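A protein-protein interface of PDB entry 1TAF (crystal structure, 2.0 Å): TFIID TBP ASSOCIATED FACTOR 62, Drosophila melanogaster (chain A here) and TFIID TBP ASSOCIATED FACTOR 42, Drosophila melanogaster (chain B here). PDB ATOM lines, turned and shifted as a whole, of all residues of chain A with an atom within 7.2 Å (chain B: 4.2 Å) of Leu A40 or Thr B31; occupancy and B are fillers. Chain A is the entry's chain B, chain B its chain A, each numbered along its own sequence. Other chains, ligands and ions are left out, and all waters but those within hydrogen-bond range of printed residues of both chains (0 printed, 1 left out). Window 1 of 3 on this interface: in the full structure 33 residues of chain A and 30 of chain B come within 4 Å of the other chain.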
ATOM      1  N   SER A   6     -21.702  -9.302   0.563  1.00  0.00           N
ATOM      2  CA  SER A   6     -21.690  -9.560  -0.857  1.00  0.00           C
ATOM      3  C   SER A   6     -23.096  -9.807  -1.368  1.00  0.00           C
ATOM      4  O   SER A   6     -23.981 -10.209  -0.621  1.00  0.00           O
ATOM      5  CB  SER A   6     -20.786 -10.753  -1.169  1.00  0.00           C
ATOM      6  OG  SER A   6     -21.251 -11.918  -0.532  1.00  0.00           O
ATOM      7  N   ILE A   7     -23.307  -9.474  -2.630  1.00  0.00           N
ATOM      8  CA  ILE A   7     -24.587  -9.671  -3.295  1.00  0.00           C
ATOM      9  C   ILE A   7     -24.818 -11.181  -3.379  1.00  0.00           C
ATOM     10  O   ILE A   7     -23.883 -11.946  -3.604  1.00  0.00           O
ATOM     11  CB  ILE A   7     -24.551  -9.037  -4.719  1.00  0.00           C
ATOM     12  CG1 ILE A   7     -24.433  -7.501  -4.620  1.00  0.00           C
ATOM     13  CG2 ILE A   7     -25.762  -9.461  -5.535  1.00  0.00           C
ATOM     14  CD1 ILE A   7     -25.609  -6.802  -3.903  1.00  0.00           C
ATOM     15  N   SER A  11     -29.718 -13.122  -6.455  1.00  0.00           N
ATOM     16  CA  SER A  11     -29.955 -11.865  -7.153  1.00  0.00           C
ATOM     17  C   SER A  11     -29.487 -11.920  -8.606  1.00  0.00           C
ATOM     18  O   SER A  11     -30.024 -11.223  -9.458  1.00  0.00           O
ATOM     19  CB  SER A  11     -29.234 -10.721  -6.435  1.00  0.00           C
ATOM     20  OG  SER A  11     -29.645 -10.635  -5.085  1.00  0.00           O
ATOM     21  N   MET A  12     -28.476 -12.737  -8.886  1.00  0.00           N
ATOM     22  CA  MET A  12     -27.943 -12.881 -10.244  1.00  0.00           C
ATOM     23  C   MET A  12     -28.972 -13.581 -11.119  1.00  0.00           C
ATOM     24  O   MET A  12     -29.067 -13.324 -12.316  1.00  0.00           O
ATOM     25  CB  MET A  12     -26.651 -13.709 -10.238  1.00  0.00           C
ATOM     26  CG  MET A  12     -25.556 -13.188  -9.320  1.00  0.00           C
ATOM     27  SD  MET A  12     -24.933 -11.577  -9.792  1.00  0.00           S
ATOM     28  CE  MET A  12     -25.879 -10.498  -8.731  1.00  0.00           C
ATOM     29  N   ILE A  15     -31.747 -11.128 -12.133  1.00  0.00           N
ATOM     30  CA  ILE A  15     -31.245 -10.263 -13.192  1.00  0.00           C
ATOM     31  C   ILE A  15     -31.223 -11.015 -14.533  1.00  0.00           C
ATOM     32  O   ILE A  15     -31.626 -10.470 -15.560  1.00  0.00           O
ATOM     33  CB  ILE A  15     -29.839  -9.707 -12.840  1.00  0.00           C
ATOM     34  CG1 ILE A  15     -29.945  -8.728 -11.669  1.00  0.00           C
ATOM     35  CG2 ILE A  15     -29.215  -9.021 -14.055  1.00  0.00           C
ATOM     36  CD1 ILE A  15     -28.605  -8.223 -11.169  1.00  0.00           C
ATOM     37  N   ALA A  33     -21.896 -13.194  -8.516  1.00  0.00           N
ATOM     38  CA  ALA A  33     -22.262 -12.494  -7.288  1.00  0.00           C
ATOM     39  C   ALA A  33     -20.996 -12.071  -6.550  1.00  0.00           C
ATOM     40  O   ALA A  33     -20.926 -10.990  -5.963  1.00  0.00           O
ATOM     41  CB  ALA A  33     -23.118 -13.388  -6.392  1.00  0.00           C
ATOM     42  N   GLU A  34     -19.988 -12.932  -6.601  1.00  0.00           N
ATOM     43  CA  GLU A  34     -18.736 -12.643  -5.948  1.00  0.00           C
ATOM     44  C   GLU A  34     -17.992 -11.543  -6.685  1.00  0.00           C
ATOM     45  O   GLU A  34     -17.496 -10.592  -6.069  1.00  0.00           O
ATOM     46  CB  GLU A  34     -17.893 -13.891  -5.904  1.00  0.00           C
ATOM     47  CG  GLU A  34     -16.646 -13.719  -5.116  1.00  0.00           C
ATOM     48  CD  GLU A  34     -15.921 -15.013  -4.984  1.00  0.00           C
ATOM     49  OE1 GLU A  34     -16.604 -16.015  -4.678  1.00  0.00           O
ATOM     50  OE2 GLU A  34     -14.690 -15.029  -5.212  1.00  0.00           O
ATOM     51  N   ASP A  35     -17.915 -11.686  -8.004  1.00  0.00           N
ATOM     52  CA  ASP A  35     -17.252 -10.714  -8.856  1.00  0.00           C
ATOM     53  C   ASP A  35     -17.864  -9.327  -8.759  1.00  0.00           C
ATOM     54  O   ASP A  35     -17.137  -8.344  -8.603  1.00  0.00           O
ATOM     55  CB  ASP A  35     -17.271 -11.192 -10.295  1.00  0.00           C
ATOM     56  CG  ASP A  35     -16.345 -12.358 -10.520  1.00  0.00           C
ATOM     57  OD1 ASP A  35     -15.554 -12.679  -9.597  1.00  0.00           O
ATOM     58  OD2 ASP A  35     -16.393 -12.947 -11.617  1.00  0.00           O
ATOM     59  N   VAL A  36     -19.192  -9.237  -8.825  1.00  0.00           N
ATOM     60  CA  VAL A  36     -19.842  -7.937  -8.732  1.00  0.00           C
ATOM     61  C   VAL A  36     -19.648  -7.293  -7.355  1.00  0.00           C
ATOM     62  O   VAL A  36     -19.536  -6.072  -7.249  1.00  0.00           O
ATOM     63  CB  VAL A  36     -21.352  -7.991  -9.112  1.00  0.00           C
ATOM     64  CG1 VAL A  36     -22.204  -8.554  -7.964  1.00  0.00           C
ATOM     65  CG2 VAL A  36     -21.830  -6.586  -9.513  1.00  0.00           C
ATOM     66  N   SER A  37     -19.578  -8.118  -6.314  1.00  0.00           N
ATOM     67  CA  SER A  37     -19.370  -7.631  -4.957  1.00  0.00           C
ATOM     68  C   SER A  37     -17.964  -7.070  -4.832  1.00  0.00           C
ATOM     69  O   SER A  37     -17.754  -6.073  -4.145  1.00  0.00           O
ATOM     70  CB  SER A  37     -19.577  -8.755  -3.964  1.00  0.00           C
ATOM     71  OG  SER A  37     -20.891  -9.241  -4.093  1.00  0.00           O
ATOM     72  N   ILE A  38     -17.006  -7.704  -5.508  1.00  0.00           N
ATOM     73  CA  ILE A  38     -15.622  -7.235  -5.495  1.00  0.00           C
ATOM     74  C   ILE A  38     -15.545  -5.887  -6.213  1.00  0.00           C
ATOM     75  O   ILE A  38     -14.824  -4.984  -5.775  1.00  0.00           O
ATOM     76  CB  ILE A  38     -14.673  -8.245  -6.183  1.00  0.00           C
ATOM     77  CG1 ILE A  38     -14.461  -9.461  -5.276  1.00  0.00           C
ATOM     78  CG2 ILE A  38     -13.339  -7.586  -6.528  1.00  0.00           C
ATOM     79  CD1 ILE A  38     -13.736 -10.619  -5.965  1.00  0.00           C
ATOM     80  N   LYS A  39     -16.295  -5.771  -7.312  1.00  0.00           N
ATOM     81  CA  LYS A  39     -16.366  -4.547  -8.112  1.00  0.00           C
ATOM     82  C   LYS A  39     -17.000  -3.424  -7.305  1.00  0.00           C
ATOM     83  O   LYS A  39     -16.526  -2.284  -7.329  1.00  0.00           O
ATOM     84  CB  LYS A  39     -17.184  -4.791  -9.372  1.00  0.00           C
ATOM     85  CG  LYS A  39     -16.386  -5.282 -10.545  1.00  0.00           C
ATOM     86  CD  LYS A  39     -15.832  -4.089 -11.313  1.00  0.00           C
ATOM     87  CE  LYS A  39     -15.037  -4.509 -12.551  1.00  0.00           C
ATOM     88  NZ  LYS A  39     -14.713  -3.310 -13.393  1.00  0.00           N
ATOM     89  N   LEU A  40     -18.073  -3.748  -6.594  1.00  0.00           N
ATOM     90  CA  LEU A  40     -18.768  -2.775  -5.749  1.00  0.00           C
ATOM     91  C   LEU A  40     -17.843  -2.193  -4.669  1.00  0.00           C
ATOM     92  O   LEU A  40     -17.839  -0.980  -4.431  1.00  0.00           O
ATOM     93  CB  LEU A  40     -19.988  -3.422  -5.087  1.00  0.00           C
ATOM     94  CG  LEU A  40     -21.214  -3.588  -5.979  1.00  0.00           C
ATOM     95  CD1 LEU A  40     -22.229  -4.487  -5.284  1.00  0.00           C
ATOM     96  CD2 LEU A  40     -21.822  -2.223  -6.285  1.00  0.00           C
ATOM     97  N   LYS A  41     -17.057  -3.058  -4.026  1.00  0.00           N
ATOM     98  CA  LYS A  41     -16.128  -2.625  -2.984  1.00  0.00           C
ATOM     99  C   LYS A  41     -15.055  -1.714  -3.587  1.00  0.00           C
ATOM    100  O   LYS A  41     -14.703  -0.705  -2.985  1.00  0.00           O
ATOM    101  CB  LYS A  41     -15.521  -3.838  -2.277  1.00  0.00           C
ATOM    102  CG  LYS A  41     -16.553  -4.672  -1.471  1.00  0.00           C
ATOM    103  CD  LYS A  41     -15.988  -6.058  -1.167  1.00  0.00           C
ATOM    104  CE  LYS A  41     -17.047  -7.068  -0.694  1.00  0.00           C
ATOM    105  NZ  LYS A  41     -17.269  -7.140   0.782  1.00  0.00           N
ATOM    106  N   ARG A  42     -14.584  -2.035  -4.796  1.00  0.00           N
ATOM    107  CA  ARG A  42     -13.587  -1.206  -5.481  1.00  0.00           C
ATOM    108  C   ARG A  42     -14.162   0.171  -5.833  1.00  0.00           C
ATOM    109  O   ARG A  42     -13.504   1.189  -5.650  1.00  0.00           O
ATOM    110  CB  ARG A  42     -13.105  -1.877  -6.763  1.00  0.00           C
ATOM    111  CG  ARG A  42     -12.294  -3.129  -6.543  1.00  0.00           C
ATOM    112  CD  ARG A  42     -11.680  -3.626  -7.841  1.00  0.00           C
ATOM    113  NE  ARG A  42     -10.956  -4.883  -7.647  1.00  0.00           N
ATOM    114  CZ  ARG A  42     -10.337  -5.560  -8.614  1.00  0.00           C
ATOM    115  NH1 ARG A  42     -10.347  -5.099  -9.861  1.00  0.00           N
ATOM    116  NH2 ARG A  42      -9.722  -6.709  -8.337  1.00  0.00           N
ATOM    117  N   ILE A  43     -15.385   0.192  -6.364  1.00  0.00           N
ATOM    118  CA  ILE A  43     -16.049   1.438  -6.735  1.00  0.00           C
ATOM    119  C   ILE A  43     -16.239   2.335  -5.505  1.00  0.00           C
ATOM    120  O   ILE A  43     -15.920   3.524  -5.540  1.00  0.00           O
ATOM    121  CB  ILE A  43     -17.428   1.154  -7.406  1.00  0.00           C
ATOM    122  CG1 ILE A  43     -17.215   0.473  -8.762  1.00  0.00           C
ATOM    123  CG2 ILE A  43     -18.222   2.450  -7.618  1.00  0.00           C
ATOM    124  CD1 ILE A  43     -18.446  -0.179  -9.324  1.00  0.00           C
ATOM    125  N   VAL A  44     -16.741   1.756  -4.418  1.00  0.00           N
ATOM    126  CA  VAL A  44     -16.966   2.495  -3.181  1.00  0.00           C
ATOM    127  C   VAL A  44     -15.638   2.998  -2.598  1.00  0.00           C
ATOM    128  O   VAL A  44     -15.534   4.146  -2.160  1.00  0.00           O
ATOM    129  CB  VAL A  44     -17.706   1.621  -2.144  1.00  0.00           C
ATOM    130  CG1 VAL A  44     -17.765   2.321  -0.792  1.00  0.00           C
ATOM    131  CG2 VAL A  44     -19.125   1.317  -2.636  1.00  0.00           C
ATOM    132  N   GLN A  45     -14.629   2.136  -2.600  1.00  0.00           N
ATOM    133  CA  GLN A  45     -13.310   2.503  -2.089  1.00  0.00           C
ATOM    134  C   GLN A  45     -12.716   3.690  -2.861  1.00  0.00           C
ATOM    135  O   GLN A  45     -12.289   4.665  -2.260  1.00  0.00           O
ATOM    136  CB  GLN A  45     -12.374   1.296  -2.163  1.00  0.00           C
ATOM    137  CG  GLN A  45     -10.974   1.530  -1.590  1.00  0.00           C
ATOM    138  CD  GLN A  45     -10.994   1.869  -0.110  1.00  0.00           C
ATOM    139  OE1 GLN A  45     -11.521   1.117   0.721  1.00  0.00           O
ATOM    140  NE2 GLN A  45     -10.421   3.014   0.225  1.00  0.00           N
ATOM    141  N   ASP A  46     -12.721   3.625  -4.188  1.00  0.00           N
ATOM    142  CA  ASP A  46     -12.176   4.704  -5.008  1.00  0.00           C
ATOM    143  C   ASP A  46     -12.971   5.984  -4.839  1.00  0.00           C
ATOM    144  O   ASP A  46     -12.395   7.072  -4.815  1.00  0.00           O
ATOM    145  CB  ASP A  46     -12.154   4.314  -6.485  1.00  0.00           C
ATOM    146  CG  ASP A  46     -11.149   3.219  -6.793  1.00  0.00           C
ATOM    147  OD1 ASP A  46     -10.212   2.982  -5.997  1.00  0.00           O
ATOM    148  OD2 ASP A  46     -11.298   2.588  -7.859  1.00  0.00           O
ATOM    149  N   ILE A  64     -19.123   8.792  -6.884  1.00  0.00           N
ATOM    150  CA  ILE A  64     -19.421   7.499  -7.502  1.00  0.00           C
ATOM    151  C   ILE A  64     -19.236   7.554  -9.022  1.00  0.00           C
ATOM    152  O   ILE A  64     -18.714   6.612  -9.624  1.00  0.00           O
ATOM    153  CB  ILE A  64     -20.841   7.028  -7.147  1.00  0.00           C
ATOM    154  CG1 ILE A  64     -20.945   6.779  -5.633  1.00  0.00           C
ATOM    155  CG2 ILE A  64     -21.203   5.767  -7.948  1.00  0.00           C
ATOM    156  CD1 ILE A  64     -20.162   5.574  -5.134  1.00  0.00           C
ATOM    157  N   SER A  67     -15.572   7.556  -9.754  1.00  0.00           N
ATOM    158  CA  SER A  67     -15.068   6.202  -9.514  1.00  0.00           C
ATOM    159  C   SER A  67     -15.408   5.257 -10.679  1.00  0.00           C
ATOM    160  O   SER A  67     -14.586   4.422 -11.074  1.00  0.00           O
ATOM    161  CB  SER A  67     -15.639   5.672  -8.194  1.00  0.00           C
ATOM    162  OG  SER A  67     -15.175   4.376  -7.901  1.00  0.00           O
ATOM    163  N   ILE B  10     -21.989  -2.713   2.690  1.00  0.00           N
ATOM    164  CA  ILE B  10     -20.662  -2.544   2.075  1.00  0.00           C
ATOM    165  C   ILE B  10     -20.148  -1.127   2.367  1.00  0.00           C
ATOM    166  O   ILE B  10     -18.981  -0.941   2.721  1.00  0.00           O
ATOM    167  CB  ILE B  10     -20.675  -2.804   0.527  1.00  0.00           C
ATOM    168  CG1 ILE B  10     -20.900  -4.301   0.233  1.00  0.00           C
ATOM    169  CG2 ILE B  10     -19.360  -2.345  -0.099  1.00  0.00           C
ATOM    170  CD1 ILE B  10     -20.899  -4.675  -1.267  1.00  0.00           C
ATOM    171  N   LEU B  27     -25.384   2.429  -7.174  1.00  0.00           N
ATOM    172  CA  LEU B  27     -24.683   1.162  -7.043  1.00  0.00           C
ATOM    173  C   LEU B  27     -25.541  -0.028  -7.446  1.00  0.00           C
ATOM    174  O   LEU B  27     -25.022  -1.024  -7.938  1.00  0.00           O
ATOM    175  CB  LEU B  27     -24.094   1.016  -5.638  1.00  0.00           C
ATOM    176  CG  LEU B  27     -22.979   2.032  -5.348  1.00  0.00           C
ATOM    177  CD1 LEU B  27     -22.664   2.058  -3.860  1.00  0.00           C
ATOM    178  CD2 LEU B  27     -21.724   1.723  -6.191  1.00  0.00           C
ATOM    179  N   LEU B  28     -26.854   0.083  -7.259  1.00  0.00           N
ATOM    180  CA  LEU B  28     -27.746  -0.996  -7.664  1.00  0.00           C
ATOM    181  C   LEU B  28     -27.791  -1.006  -9.196  1.00  0.00           C
ATOM    182  O   LEU B  28     -27.814  -2.062  -9.827  1.00  0.00           O
ATOM    183  CB  LEU B  28     -29.153  -0.795  -7.083  1.00  0.00           C
ATOM    184  CG  LEU B  28     -29.296  -1.117  -5.593  1.00  0.00           C
ATOM    185  CD1 LEU B  28     -30.637  -0.657  -5.062  1.00  0.00           C
ATOM    186  CD2 LEU B  28     -29.127  -2.600  -5.384  1.00  0.00           C
ATOM    187  N   GLU B  29     -27.745   0.183  -9.787  1.00  0.00           N
ATOM    188  CA  GLU B  29     -27.780   0.322 -11.233  1.00  0.00           C
ATOM    189  C   GLU B  29     -26.505  -0.229 -11.843  1.00  0.00           C
ATOM    190  O   GLU B  29     -26.533  -0.884 -12.890  1.00  0.00           O
ATOM    191  CB  GLU B  29     -28.012   1.782 -11.596  1.00  0.00           C
ATOM    192  CG  GLU B  29     -29.432   2.184 -11.207  1.00  0.00           C
ATOM    193  CD  GLU B  29     -29.671   3.677 -11.122  1.00  0.00           C
ATOM    194  OE1 GLU B  29     -28.755   4.468 -11.445  1.00  0.00           O
ATOM    195  OE2 GLU B  29     -30.798   4.055 -10.712  1.00  0.00           O
ATOM    196  N   PHE B  30     -25.391   0.004 -11.159  1.00  0.00           N
ATOM    197  CA  PHE B  30     -24.113  -0.510 -11.613  1.00  0.00           C
ATOM    198  C   PHE B  30     -24.164  -2.027 -11.556  1.00  0.00           C
ATOM    199  O   PHE B  30     -23.710  -2.690 -12.476  1.00  0.00           O
ATOM    200  CB  PHE B  30     -22.949  -0.048 -10.731  1.00  0.00           C
ATOM    201  CG  PHE B  30     -21.697  -0.865 -10.943  1.00  0.00           C
ATOM    202  CD1 PHE B  30     -20.911  -0.667 -12.084  1.00  0.00           C
ATOM    203  CD2 PHE B  30     -21.382  -1.913 -10.079  1.00  0.00           C
ATOM    204  CE1 PHE B  30     -19.843  -1.507 -12.367  1.00  0.00           C
ATOM    205  CE2 PHE B  30     -20.318  -2.757 -10.353  1.00  0.00           C
ATOM    206  CZ  PHE B  30     -19.549  -2.555 -11.501  1.00  0.00           C
ATOM    207  N   THR B  31     -24.651  -2.561 -10.440  1.00  0.00           N
ATOM    208  CA  THR B  31     -24.759  -4.002 -10.253  1.00  0.00           C
ATOM    209  C   THR B  31     -25.501  -4.627 -11.433  1.00  0.00           C
ATOM    210  O   THR B  31     -25.024  -5.583 -12.041  1.00  0.00           O
ATOM    211  CB  THR B  31     -25.525  -4.333  -8.960  1.00  0.00           C
ATOM    212  OG1 THR B  31     -24.826  -3.779  -7.842  1.00  0.00           O
ATOM    213  CG2 THR B  31     -25.656  -5.834  -8.769  1.00  0.00           C
ATOM    214  N   PHE B  32     -26.636  -4.032 -11.787  1.00  0.00           N
ATOM    215  CA  PHE B  32     -27.455  -4.527 -12.877  1.00  0.00           C
ATOM    216  C   PHE B  32     -26.709  -4.450 -14.200  1.00  0.00           C
ATOM    217  O   PHE B  32     -26.673  -5.408 -14.967  1.00  0.00           O
ATOM    218  CB  PHE B  32     -28.759  -3.727 -12.944  1.00  0.00           C
ATOM    219  CG  PHE B  32     -29.737  -4.239 -13.968  1.00  0.00           C
ATOM    220  CD1 PHE B  32     -30.622  -5.269 -13.648  1.00  0.00           C
ATOM    221  CD2 PHE B  32     -29.753  -3.712 -15.263  1.00  0.00           C
ATOM    222  CE1 PHE B  32     -31.500  -5.764 -14.600  1.00  0.00           C
ATOM    223  CE2 PHE B  32     -30.626  -4.202 -16.216  1.00  0.00           C
ATOM    224  CZ  PHE B  32     -31.498  -5.231 -15.884  1.00  0.00           C
ATOM    225  N   ARG B  33     -26.076  -3.317 -14.438  1.00  0.00           N
ATOM    226  CA  ARG B  33     -25.334  -3.087 -15.664  1.00  0.00           C
ATOM    227  C   ARG B  33     -24.174  -4.062 -15.834  1.00  0.00           C
ATOM    228  O   ARG B  33     -23.964  -4.590 -16.923  1.00  0.00           O
ATOM    229  CB  ARG B  33     -24.804  -1.660 -15.648  1.00  0.00           C
ATOM    230  CG  ARG B  33     -24.549  -1.044 -16.998  1.00  0.00           C
ATOM    231  CD  ARG B  33     -24.080   0.403 -16.830  1.00  0.00           C
ATOM    232  NE  ARG B  33     -24.980   1.175 -15.979  1.00  0.00           N
ATOM    233  CZ  ARG B  33     -24.609   1.834 -14.881  1.00  0.00           C
ATOM    234  NH1 ARG B  33     -23.344   1.837 -14.472  1.00  0.00           N
ATOM    235  NH2 ARG B  33     -25.520   2.492 -14.179  1.00  0.00           N
ATOM    236  N   TYR B  34     -23.433  -4.299 -14.754  1.00  0.00           N
ATOM    237  CA  TYR B  34     -22.278  -5.191 -14.779  1.00  0.00           C
ATOM    238  C   TYR B  34     -22.713  -6.628 -15.031  1.00  0.00           C
ATOM    239  O   TYR B  34     -22.179  -7.298 -15.905  1.00  0.00           O
ATOM    240  CB  TYR B  34     -21.482  -5.099 -13.459  1.00  0.00           C
ATOM    241  CG  TYR B  34     -20.324  -6.075 -13.363  1.00  0.00           C
ATOM    242  CD1 TYR B  34     -19.091  -5.768 -13.917  1.00  0.00           C
ATOM    243  CD2 TYR B  34     -20.493  -7.342 -12.798  1.00  0.00           C
ATOM    244  CE1 TYR B  34     -18.052  -6.704 -13.932  1.00  0.00           C
ATOM    245  CE2 TYR B  34     -19.471  -8.284 -12.805  1.00  0.00           C
ATOM    246  CZ  TYR B  34     -18.253  -7.954 -13.381  1.00  0.00           C
ATOM    247  OH  TYR B  34     -17.243  -8.888 -13.449  1.00  0.00           O
ATOM    248  N   VAL B  35     -23.676  -7.099 -14.251  1.00  0.00           N
ATOM    249  CA  VAL B  35     -24.164  -8.459 -14.390  1.00  0.00           C
ATOM    250  C   VAL B  35     -24.786  -8.685 -15.765  1.00  0.00           C
ATOM    251  O   VAL B  35     -24.487  -9.670 -16.427  1.00  0.00           O
ATOM    252  CB  VAL B  35     -25.153  -8.799 -13.268  1.00  0.00           C
ATOM    253  CG1 VAL B  35     -25.780 -10.157 -13.501  1.00  0.00           C
ATOM    254  CG2 VAL B  35     -24.428  -8.779 -11.931  1.00  0.00           C
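OG1 of Thr B31 sits at hydrogen-bond distance from O of Leu B27, at 2.8 Å.
The side-chain sulfur (SD) of Met A12 sits at hydrogen-bond distance from the backbone NH (N) of Ala A33.
The backbone carbonyl oxygen (O) of Ile A43 is in hydrogen-bond range of the side-chain hydroxyl (OG) of Ser A67 (2.6 Å).
Of the 10 printed residues of chain B, 6 touch a printed residue of chain A.
Printed residues of chain B that touch a printed residue of chain A: Ile B10, Leu B27, Phe B30, Thr B31, Tyr B34 and Val B35.
Of the 21 printed residues of chain A, 9 touch a printed residue of chain B.
Hydrophobic or aromatic side chains of chain A within 4 Å of the printed part of chain B: Met A12, Ile A15, Val A36, Leu A40, Ile A43 and Val A44.
Among the printed residues, no Asp or Glu carboxylate lies within 4 Å of a Lys or Arg side-chain nitrogen of the other chain.
Among the printed residues, merely in contact across the chains: Ile A43 with Phe B30, Met A12 with Val B35, Val A36 with Tyr B34, Ile A15 with Val B35, Leu A40 with Thr B31, Leu A40 with Leu B27, Val A44 with Leu B27, Leu A40 with Phe B30, Ile A43 with Leu B27, Lys A39 with Phe B30, Lys A41 with Ile B10, Asp A35 with Tyr B34, Val A36 with Thr B31 and Lys A39 with Tyr B34.
Ser A11 touches none of the printed residues of chain B.
Of the printed residues of chain B, Ile A15 touches Val B35 (3.7 Å).
Printed residues of chain B within 4 Å of Asp A35: Tyr B34 (3.9 Å).
Printed residues of chain B within 4 Å of Leu A40: Leu B27 (3.8 Å), Phe B30 (3.8 Å) and Thr B31 (3.7 Å).
Printed residues of chain B within 4 Å of Lys A41: Ile B10 (3.9 Å).
Printed residues of chain B within 4 Å of Ile A43: Leu B27 (3.9 Å) and Phe B30 (3.3 Å).
Of the printed residues of chain A, Thr B31 touches Val A36 (3.97 Å) and Leu A40 (3.7 Å).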
